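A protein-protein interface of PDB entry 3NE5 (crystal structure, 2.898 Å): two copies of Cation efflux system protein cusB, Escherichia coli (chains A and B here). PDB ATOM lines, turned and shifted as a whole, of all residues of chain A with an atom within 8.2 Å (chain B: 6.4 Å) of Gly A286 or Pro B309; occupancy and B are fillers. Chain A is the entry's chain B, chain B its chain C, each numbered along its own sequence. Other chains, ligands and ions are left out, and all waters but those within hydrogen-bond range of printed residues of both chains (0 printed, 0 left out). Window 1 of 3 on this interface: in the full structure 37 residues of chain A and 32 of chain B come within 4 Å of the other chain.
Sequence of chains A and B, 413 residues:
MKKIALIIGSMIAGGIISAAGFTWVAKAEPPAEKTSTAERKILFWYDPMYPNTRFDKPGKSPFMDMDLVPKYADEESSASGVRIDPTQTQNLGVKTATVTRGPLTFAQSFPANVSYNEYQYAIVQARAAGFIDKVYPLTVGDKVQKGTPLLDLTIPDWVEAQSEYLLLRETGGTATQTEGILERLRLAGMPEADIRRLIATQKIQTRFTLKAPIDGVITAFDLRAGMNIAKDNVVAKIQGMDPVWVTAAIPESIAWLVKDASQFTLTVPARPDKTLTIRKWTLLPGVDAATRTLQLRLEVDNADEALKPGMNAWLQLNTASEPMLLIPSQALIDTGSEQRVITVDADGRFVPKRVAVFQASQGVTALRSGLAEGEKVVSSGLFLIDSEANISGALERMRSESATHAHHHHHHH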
ATOM      1  N   GLU A 252      11.792  15.238   4.571  1.00  0.00           N
ATOM      2  CA  GLU A 252      10.794  14.742   3.630  1.00  0.00           C
ATOM      3  C   GLU A 252       9.922  15.836   3.011  1.00  0.00           C
ATOM      4  O   GLU A 252       9.525  15.739   1.851  1.00  0.00           O
ATOM      5  CB  GLU A 252       9.917  13.699   4.325  1.00  0.00           C
ATOM      6  CG  GLU A 252       8.433  13.902   4.118  1.00  0.00           C
ATOM      7  CD  GLU A 252       7.607  13.285   5.222  1.00  0.00           C
ATOM      8  OE1 GLU A 252       6.976  14.042   5.988  1.00  0.00           O
ATOM      9  OE2 GLU A 252       7.599  12.044   5.334  1.00  0.00           O
ATOM     10  N   LEU A 283      19.025   9.663  -5.136  1.00  0.00           N
ATOM     11  CA  LEU A 283      18.032   9.844  -4.087  1.00  0.00           C
ATOM     12  C   LEU A 283      17.341   8.517  -3.783  1.00  0.00           C
ATOM     13  O   LEU A 283      16.448   8.094  -4.513  1.00  0.00           O
ATOM     14  CB  LEU A 283      17.007  10.896  -4.511  1.00  0.00           C
ATOM     15  CG  LEU A 283      15.961  11.316  -3.478  1.00  0.00           C
ATOM     16  CD1 LEU A 283      16.627  11.862  -2.228  1.00  0.00           C
ATOM     17  CD2 LEU A 283      15.015  12.345  -4.076  1.00  0.00           C
ATOM     18  N   LEU A 284      17.761   7.869  -2.701  1.00  0.00           N
ATOM     19  CA  LEU A 284      17.281   6.531  -2.355  1.00  0.00           C
ATOM     20  C   LEU A 284      15.758   6.438  -2.218  1.00  0.00           C
ATOM     21  O   LEU A 284      15.097   7.418  -1.870  1.00  0.00           O
ATOM     22  CB  LEU A 284      17.964   6.033  -1.081  1.00  0.00           C
ATOM     23  CG  LEU A 284      19.490   5.986  -1.156  1.00  0.00           C
ATOM     24  CD1 LEU A 284      20.077   5.514   0.164  1.00  0.00           C
ATOM     25  CD2 LEU A 284      19.952   5.095  -2.305  1.00  0.00           C
ATOM     26  N   PRO A 285      15.205   5.245  -2.497  1.00  0.00           N
ATOM     27  CA  PRO A 285      13.769   4.937  -2.501  1.00  0.00           C
ATOM     28  C   PRO A 285      13.103   5.038  -1.133  1.00  0.00           C
ATOM     29  O   PRO A 285      11.915   5.333  -1.064  1.00  0.00           O
ATOM     30  CB  PRO A 285      13.733   3.482  -2.990  1.00  0.00           C
ATOM     31  CG  PRO A 285      15.095   2.954  -2.681  1.00  0.00           C
ATOM     32  CD  PRO A 285      15.987   4.102  -2.997  1.00  0.00           C
ATOM     33  N   GLY A 286      13.851   4.791  -0.065  1.00  0.00           N
ATOM     34  CA  GLY A 286      13.282   4.815   1.269  1.00  0.00           C
ATOM     35  C   GLY A 286      13.719   5.998   2.108  1.00  0.00           C
ATOM     36  O   GLY A 286      14.828   6.506   1.960  1.00  0.00           O
ATOM     37  N   VAL A 287      12.835   6.442   2.996  1.00  0.00           N
ATOM     38  CA  VAL A 287      13.166   7.520   3.919  1.00  0.00           C
ATOM     39  C   VAL A 287      13.206   6.999   5.351  1.00  0.00           C
ATOM     40  O   VAL A 287      12.358   6.205   5.758  1.00  0.00           O
ATOM     41  CB  VAL A 287      12.186   8.713   3.805  1.00  0.00           C
ATOM     42  CG1 VAL A 287      11.772   8.929   2.355  1.00  0.00           C
ATOM     43  CG2 VAL A 287      10.970   8.513   4.693  1.00  0.00           C
ATOM     44  N   ASP A 288      14.208   7.441   6.104  1.00  0.00           N
ATOM     45  CA  ASP A 288      14.351   7.050   7.498  1.00  0.00           C
ATOM     46  C   ASP A 288      13.064   7.369   8.241  1.00  0.00           C
ATOM     47  O   ASP A 288      12.434   8.398   7.993  1.00  0.00           O
ATOM     48  CB  ASP A 288      15.533   7.781   8.138  1.00  0.00           C
ATOM     49  CG  ASP A 288      15.792   7.339   9.562  1.00  0.00           C
ATOM     50  OD1 ASP A 288      15.573   6.147   9.868  1.00  0.00           O
ATOM     51  OD2 ASP A 288      16.222   8.181  10.378  1.00  0.00           O
ATOM     52  N   ALA A 289      12.671   6.484   9.149  1.00  0.00           N
ATOM     53  CA  ALA A 289      11.413   6.644   9.867  1.00  0.00           C
ATOM     54  C   ALA A 289      11.587   7.355  11.208  1.00  0.00           C
ATOM     55  O   ALA A 289      10.741   8.158  11.594  1.00  0.00           O
ATOM     56  CB  ALA A 289      10.728   5.302  10.050  1.00  0.00           C
ATOM     57  N   ARG A 292      12.043  11.572   9.855  1.00  0.00           N
ATOM     58  CA  ARG A 292      11.415  11.452   8.548  1.00  0.00           C
ATOM     59  C   ARG A 292      12.234  12.211   7.519  1.00  0.00           C
ATOM     60  O   ARG A 292      11.932  13.355   7.197  1.00  0.00           O
ATOM     61  CB  ARG A 292       9.991  11.994   8.598  1.00  0.00           C
ATOM     62  CG  ARG A 292       9.175  11.432   9.744  1.00  0.00           C
ATOM     63  CD  ARG A 292       8.762  10.007   9.455  1.00  0.00           C
ATOM     64  NE  ARG A 292       7.985   9.432  10.547  1.00  0.00           N
ATOM     65  CZ  ARG A 292       7.230   8.346  10.428  1.00  0.00           C
ATOM     66  NH1 ARG A 292       7.141   7.722   9.263  1.00  0.00           N
ATOM     67  NH2 ARG A 292       6.555   7.889  11.471  1.00  0.00           N
ATOM     68  N   THR A 293      13.276  11.567   7.009  1.00  0.00           N
ATOM     69  CA  THR A 293      14.212  12.231   6.114  1.00  0.00           C
ATOM     70  C   THR A 293      14.508  11.394   4.882  1.00  0.00           C
ATOM     71  O   THR A 293      14.692  10.181   4.970  1.00  0.00           O
ATOM     72  CB  THR A 293      15.551  12.514   6.817  1.00  0.00           C
ATOM     73  OG1 THR A 293      16.164  11.271   7.187  1.00  0.00           O
ATOM     74  CG2 THR A 293      15.336  13.358   8.063  1.00  0.00           C
ATOM     75  N   LEU A 294      14.557  12.056   3.732  1.00  0.00           N
ATOM     76  CA  LEU A 294      15.007  11.426   2.505  1.00  0.00           C
ATOM     77  C   LEU A 294      16.488  11.107   2.657  1.00  0.00           C
ATOM     78  O   LEU A 294      17.188  11.749   3.439  1.00  0.00           O
ATOM     79  CB  LEU A 294      14.800  12.371   1.323  1.00  0.00           C
ATOM     80  CG  LEU A 294      13.374  12.852   1.076  1.00  0.00           C
ATOM     81  CD1 LEU A 294      13.389  14.106   0.224  1.00  0.00           C
ATOM     82  CD2 LEU A 294      12.559  11.761   0.408  1.00  0.00           C
ATOM     83  N   GLN A 295      16.966  10.114   1.915  1.00  0.00           N
ATOM     84  CA  GLN A 295      18.378   9.750   1.963  1.00  0.00           C
ATOM     85  C   GLN A 295      19.042   9.949   0.606  1.00  0.00           C
ATOM     86  O   GLN A 295      18.741   9.249  -0.358  1.00  0.00           O
ATOM     87  CB  GLN A 295      18.555   8.306   2.438  1.00  0.00           C
ATOM     88  CG  GLN A 295      17.977   8.026   3.818  1.00  0.00           C
ATOM     89  CD  GLN A 295      18.657   8.824   4.917  1.00  0.00           C
ATOM     90  OE1 GLN A 295      19.884   8.912   4.969  1.00  0.00           O
ATOM     91  NE2 GLN A 295      17.859   9.403   5.807  1.00  0.00           N
ATOM     92  N   LEU A 296      19.947  10.916   0.542  1.00  0.00           N
ATOM     93  CA  LEU A 296      20.645  11.230  -0.695  1.00  0.00           C
ATOM     94  C   LEU A 296      22.102  10.798  -0.584  1.00  0.00           C
ATOM     95  O   LEU A 296      22.830  11.262   0.293  1.00  0.00           O
ATOM     96  CB  LEU A 296      20.541  12.729  -0.988  1.00  0.00           C
ATOM     97  CG  LEU A 296      21.036  13.243  -2.338  1.00  0.00           C
ATOM     98  CD1 LEU A 296      20.453  14.617  -2.622  1.00  0.00           C
ATOM     99  CD2 LEU A 296      22.552  13.284  -2.377  1.00  0.00           C
ATOM    100  N   VAL B 114       3.726   5.523   5.410  1.00  0.00           N
ATOM    101  CA  VAL B 114       3.910   4.907   4.106  1.00  0.00           C
ATOM    102  C   VAL B 114       4.880   3.760   4.318  1.00  0.00           C
ATOM    103  O   VAL B 114       5.973   3.960   4.839  1.00  0.00           O
ATOM    104  CB  VAL B 114       4.493   5.906   3.101  1.00  0.00           C
ATOM    105  CG1 VAL B 114       4.681   5.257   1.740  1.00  0.00           C
ATOM    106  CG2 VAL B 114       3.594   7.121   2.995  1.00  0.00           C
ATOM    107  N   SER B 115       4.471   2.553   3.946  1.00  0.00           N
ATOM    108  CA  SER B 115       5.305   1.381   4.179  1.00  0.00           C
ATOM    109  C   SER B 115       5.367   0.486   2.950  1.00  0.00           C
ATOM    110  O   SER B 115       4.618   0.673   1.991  1.00  0.00           O
ATOM    111  CB  SER B 115       4.795   0.589   5.386  1.00  0.00           C
ATOM    112  OG  SER B 115       3.412   0.307   5.264  1.00  0.00           O
ATOM    113  N   TYR B 116       6.272  -0.487   2.991  1.00  0.00           N
ATOM    114  CA  TYR B 116       6.460  -1.409   1.881  1.00  0.00           C
ATOM    115  C   TYR B 116       5.249  -2.316   1.693  1.00  0.00           C
ATOM    116  O   TYR B 116       4.586  -2.695   2.659  1.00  0.00           O
ATOM    117  CB  TYR B 116       7.708  -2.264   2.104  1.00  0.00           C
ATOM    118  CG  TYR B 116       9.013  -1.513   1.977  1.00  0.00           C
ATOM    119  CD1 TYR B 116       9.748  -1.163   3.101  1.00  0.00           C
ATOM    120  CD2 TYR B 116       9.516  -1.160   0.731  1.00  0.00           C
ATOM    121  CE1 TYR B 116      10.945  -0.482   2.990  1.00  0.00           C
ATOM    122  CE2 TYR B 116      10.711  -0.478   0.609  1.00  0.00           C
ATOM    123  CZ  TYR B 116      11.422  -0.141   1.741  1.00  0.00           C
ATOM    124  OH  TYR B 116      12.613   0.538   1.623  1.00  0.00           O
ATOM    125  N   ASN B 117       4.967  -2.659   0.440  1.00  0.00           N
ATOM    126  CA  ASN B 117       3.897  -3.594   0.123  1.00  0.00           C
ATOM    127  C   ASN B 117       4.323  -5.007   0.483  1.00  0.00           C
ATOM    128  O   ASN B 117       5.215  -5.575  -0.146  1.00  0.00           O
ATOM    129  CB  ASN B 117       3.546  -3.516  -1.362  1.00  0.00           C
ATOM    130  CG  ASN B 117       2.297  -4.297  -1.706  1.00  0.00           C
ATOM    131  OD1 ASN B 117       1.970  -5.288  -1.054  1.00  0.00           O
ATOM    132  ND2 ASN B 117       1.593  -3.857  -2.740  1.00  0.00           N
ATOM    133  N   GLY B 141      19.166  -0.645   0.741  1.00  0.00           N
ATOM    134  CA  GLY B 141      18.717   0.712   0.488  1.00  0.00           C
ATOM    135  C   GLY B 141      18.606   1.009  -0.994  1.00  0.00           C
ATOM    136  O   GLY B 141      18.023   2.014  -1.393  1.00  0.00           O
ATOM    137  N   VAL B 217      12.836  -2.709  -3.409  1.00  0.00           N
ATOM    138  CA  VAL B 217      13.969  -2.151  -2.683  1.00  0.00           C
ATOM    139  C   VAL B 217      14.668  -3.215  -1.849  1.00  0.00           C
ATOM    140  O   VAL B 217      14.018  -4.008  -1.169  1.00  0.00           O
ATOM    141  CB  VAL B 217      13.525  -1.016  -1.744  1.00  0.00           C
ATOM    142  CG1 VAL B 217      14.731  -0.403  -1.050  1.00  0.00           C
ATOM    143  CG2 VAL B 217      12.758   0.040  -2.518  1.00  0.00           C
ATOM    144  N   GLY B 240       8.561  -4.461  -2.572  1.00  0.00           N
ATOM    145  CA  GLY B 240       8.056  -3.555  -3.592  1.00  0.00           C
ATOM    146  C   GLY B 240       7.149  -2.448  -3.083  1.00  0.00           C
ATOM    147  O   GLY B 240       6.492  -2.593  -2.053  1.00  0.00           O
ATOM    148  N   MET B 241       7.098  -1.343  -3.825  1.00  0.00           N
ATOM    149  CA  MET B 241       6.346  -0.162  -3.404  1.00  0.00           C
ATOM    150  C   MET B 241       5.418   0.439  -4.468  1.00  0.00           C
ATOM    151  O   MET B 241       4.937   1.552  -4.295  1.00  0.00           O
ATOM    152  CB  MET B 241       7.314   0.920  -2.911  1.00  0.00           C
ATOM    153  CG  MET B 241       8.512   1.095  -3.816  1.00  0.00           C
ATOM    154  SD  MET B 241       9.788   2.145  -3.108  1.00  0.00           S
ATOM    155  CE  MET B 241       9.190   3.762  -3.590  1.00  0.00           C
ATOM    156  N   VAL B 244       1.796   0.890  -3.293  1.00  0.00           N
ATOM    157  CA  VAL B 244       2.345   1.172  -1.977  1.00  0.00           C
ATOM    158  C   VAL B 244       1.293   1.090  -0.867  1.00  0.00           C
ATOM    159  O   VAL B 244       0.098   1.309  -1.099  1.00  0.00           O
ATOM    160  CB  VAL B 244       3.014   2.541  -1.945  1.00  0.00           C
ATOM    161  CG1 VAL B 244       1.959   3.631  -2.057  1.00  0.00           C
ATOM    162  CG2 VAL B 244       3.853   2.711  -0.703  1.00  0.00           C
ATOM    163  N   ASN B 302       1.209   3.974  -6.959  1.00  0.00           N
ATOM    164  CA  ASN B 302       2.503   4.619  -6.793  1.00  0.00           C
ATOM    165  C   ASN B 302       3.435   4.291  -7.952  1.00  0.00           C
ATOM    166  O   ASN B 302       4.616   4.004  -7.752  1.00  0.00           O
ATOM    167  CB  ASN B 302       3.131   4.205  -5.460  1.00  0.00           C
ATOM    168  CG  ASN B 302       4.309   5.069  -5.075  1.00  0.00           C
ATOM    169  OD1 ASN B 302       5.313   4.575  -4.562  1.00  0.00           O
ATOM    170  ND2 ASN B 302       4.196   6.370  -5.324  1.00  0.00           N
ATOM    171  N   LEU B 307       5.707   8.147  -3.520  1.00  0.00           N
ATOM    172  CA  LEU B 307       5.511   7.776  -2.123  1.00  0.00           C
ATOM    173  C   LEU B 307       6.578   6.802  -1.644  1.00  0.00           C
ATOM    174  O   LEU B 307       6.588   5.633  -2.024  1.00  0.00           O
ATOM    175  CB  LEU B 307       4.121   7.179  -1.909  1.00  0.00           C
ATOM    176  CG  LEU B 307       2.994   8.161  -1.597  1.00  0.00           C
ATOM    177  CD1 LEU B 307       2.905   9.246  -2.655  1.00  0.00           C
ATOM    178  CD2 LEU B 307       1.679   7.412  -1.470  1.00  0.00           C
ATOM    179  N   LYS B 308       7.472   7.300  -0.801  1.00  0.00           N
ATOM    180  CA  LYS B 308       8.567   6.501  -0.280  1.00  0.00           C
ATOM    181  C   LYS B 308       8.216   5.946   1.091  1.00  0.00           C
ATOM    182  O   LYS B 308       7.726   6.674   1.949  1.00  0.00           O
ATOM    183  CB  LYS B 308       9.829   7.356  -0.174  1.00  0.00           C
ATOM    184  CG  LYS B 308      10.355   7.863  -1.502  1.00  0.00           C
ATOM    185  CD  LYS B 308      11.490   8.846  -1.285  1.00  0.00           C
ATOM    186  CE  LYS B 308      12.420   8.891  -2.485  1.00  0.00           C
ATOM    187  NZ  LYS B 308      11.696   9.159  -3.757  1.00  0.00           N
ATOM    188  N   PRO B 309       8.455   4.646   1.298  1.00  0.00           N
ATOM    189  CA  PRO B 309       8.244   4.054   2.620  1.00  0.00           C
ATOM    190  C   PRO B 309       8.989   4.838   3.698  1.00  0.00           C
ATOM    191  O   PRO B 309      10.145   5.212   3.507  1.00  0.00           O
ATOM    192  CB  PRO B 309       8.837   2.654   2.463  1.00  0.00           C
ATOM    193  CG  PRO B 309       8.638   2.338   1.022  1.00  0.00           C
ATOM    194  CD  PRO B 309       8.835   3.638   0.294  1.00  0.00           C
ATOM    195  N   GLY B 310       8.317   5.086   4.818  1.00  0.00           N
ATOM    196  CA  GLY B 310       8.883   5.868   5.901  1.00  0.00           C
ATOM    197  C   GLY B 310       8.315   7.273   5.930  1.00  0.00           C
ATOM    198  O   GLY B 310       8.506   8.015   6.893  1.00  0.00           O
ATOM    199  N   MET B 311       7.620   7.639   4.860  1.00  0.00           N
ATOM    200  CA  MET B 311       7.003   8.955   4.757  1.00  0.00           C
ATOM    201  C   MET B 311       5.791   9.090   5.663  1.00  0.00           C
ATOM    202  O   MET B 311       5.190   8.097   6.071  1.00  0.00           O
ATOM    203  CB  MET B 311       6.582   9.238   3.316  1.00  0.00           C
ATOM    204  CG  MET B 311       7.679   9.785   2.433  1.00  0.00           C
ATOM    205  SD  MET B 311       7.027  10.251   0.824  1.00  0.00           S
ATOM    206  CE  MET B 311       8.448  11.075   0.128  1.00  0.00           C
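The backbone carbonyl oxygen (O) of Pro B309 is in hydrogen-bond range of the backbone NH (N) of Val A287 (3.0 Å). The guanidinium group (NH1) of Arg A292 sits at hydrogen-bond distance from the backbone carbonyl oxygen (O) of Gly B310, 2.8 Å away.
N of Glu A252 sits at hydrogen-bond distance from O of Arg A292 (3.2 Å). N of Leu A284 lies within hydrogen-bond range of O of Gln A295 (2.9 Å). The backbone carbonyl oxygen (O) of Ala A289 sits at hydrogen-bond distance from the guanidinium group (NE) of Arg A292 (3.2 Å). The backbone carbonyl oxygen (O) of Val B114 sits at hydrogen-bond distance from the backbone NH (N) of Gly B310, 2.6 Å away. The backbone NH (N) of Val B114 lies within hydrogen-bond range of the backbone carbonyl oxygen (O) of Met B311. The backbone NH (N) of Lys B308 sits at hydrogen-bond distance from the side-chain sulfur (SD) of Met B311.
Among the printed residues, merely in contact across the chains: Pro A285 with Lys B308 (3.0 Å), Leu A284 with Lys B308 (3.1 Å), Val A287 with Gly B310 (3.2 Å), Glu A252 with Met B311 (3.2 Å), Pro A285 with Gly B141 (3.3 Å), Val A287 with Met B311 (3.5 Å), Leu A294 with Lys B308 (3.5 Å), Val A287 with Lys B308 (3.6 Å), Pro A285 with Val B217 (3.6 Å), Leu A284 with Gly B141 (3.7 Å), Arg A292 with Met B311 (3.8 Å), Pro A285 with Pro B309 (3.8 Å) and Gly A286 with Pro B309 (3.9 Å).
Of chain B, only Pro B309 comes within 4 Å of Gly A286. Of the printed residues of chain A, Val B217 touches Pro A285 (3.6 Å). Of the printed residues of chain B, Arg A292 touches Gly B310 (2.8 Å) and Met B311 (3.8 Å). Tyr B116 touches none of the printed residues of chain A. The nearest residue of chain B that does not touch Gly A286 is Tyr B116 (4.3 Å). The nearest printed residue of chain A that does not touch Gly B310 is Asp A288 (4.1 Å).
Hydrophobic or aromatic side chains of chain A within 4 Å of the printed part of chain B: Leu A284, Pro A285, Val A287 and Leu A294. Hydrophobic or aromatic side chains of chain B that line the printed part of chain A: Val B217, Pro B309 and Met B311. Among the printed residues, 15 pairs touch across the chains. Among the printed residues, no Asp or Glu carboxylate lies within 4 Å of a Lys or Arg side-chain nitrogen of the other chain.
No position is printed for both chains.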
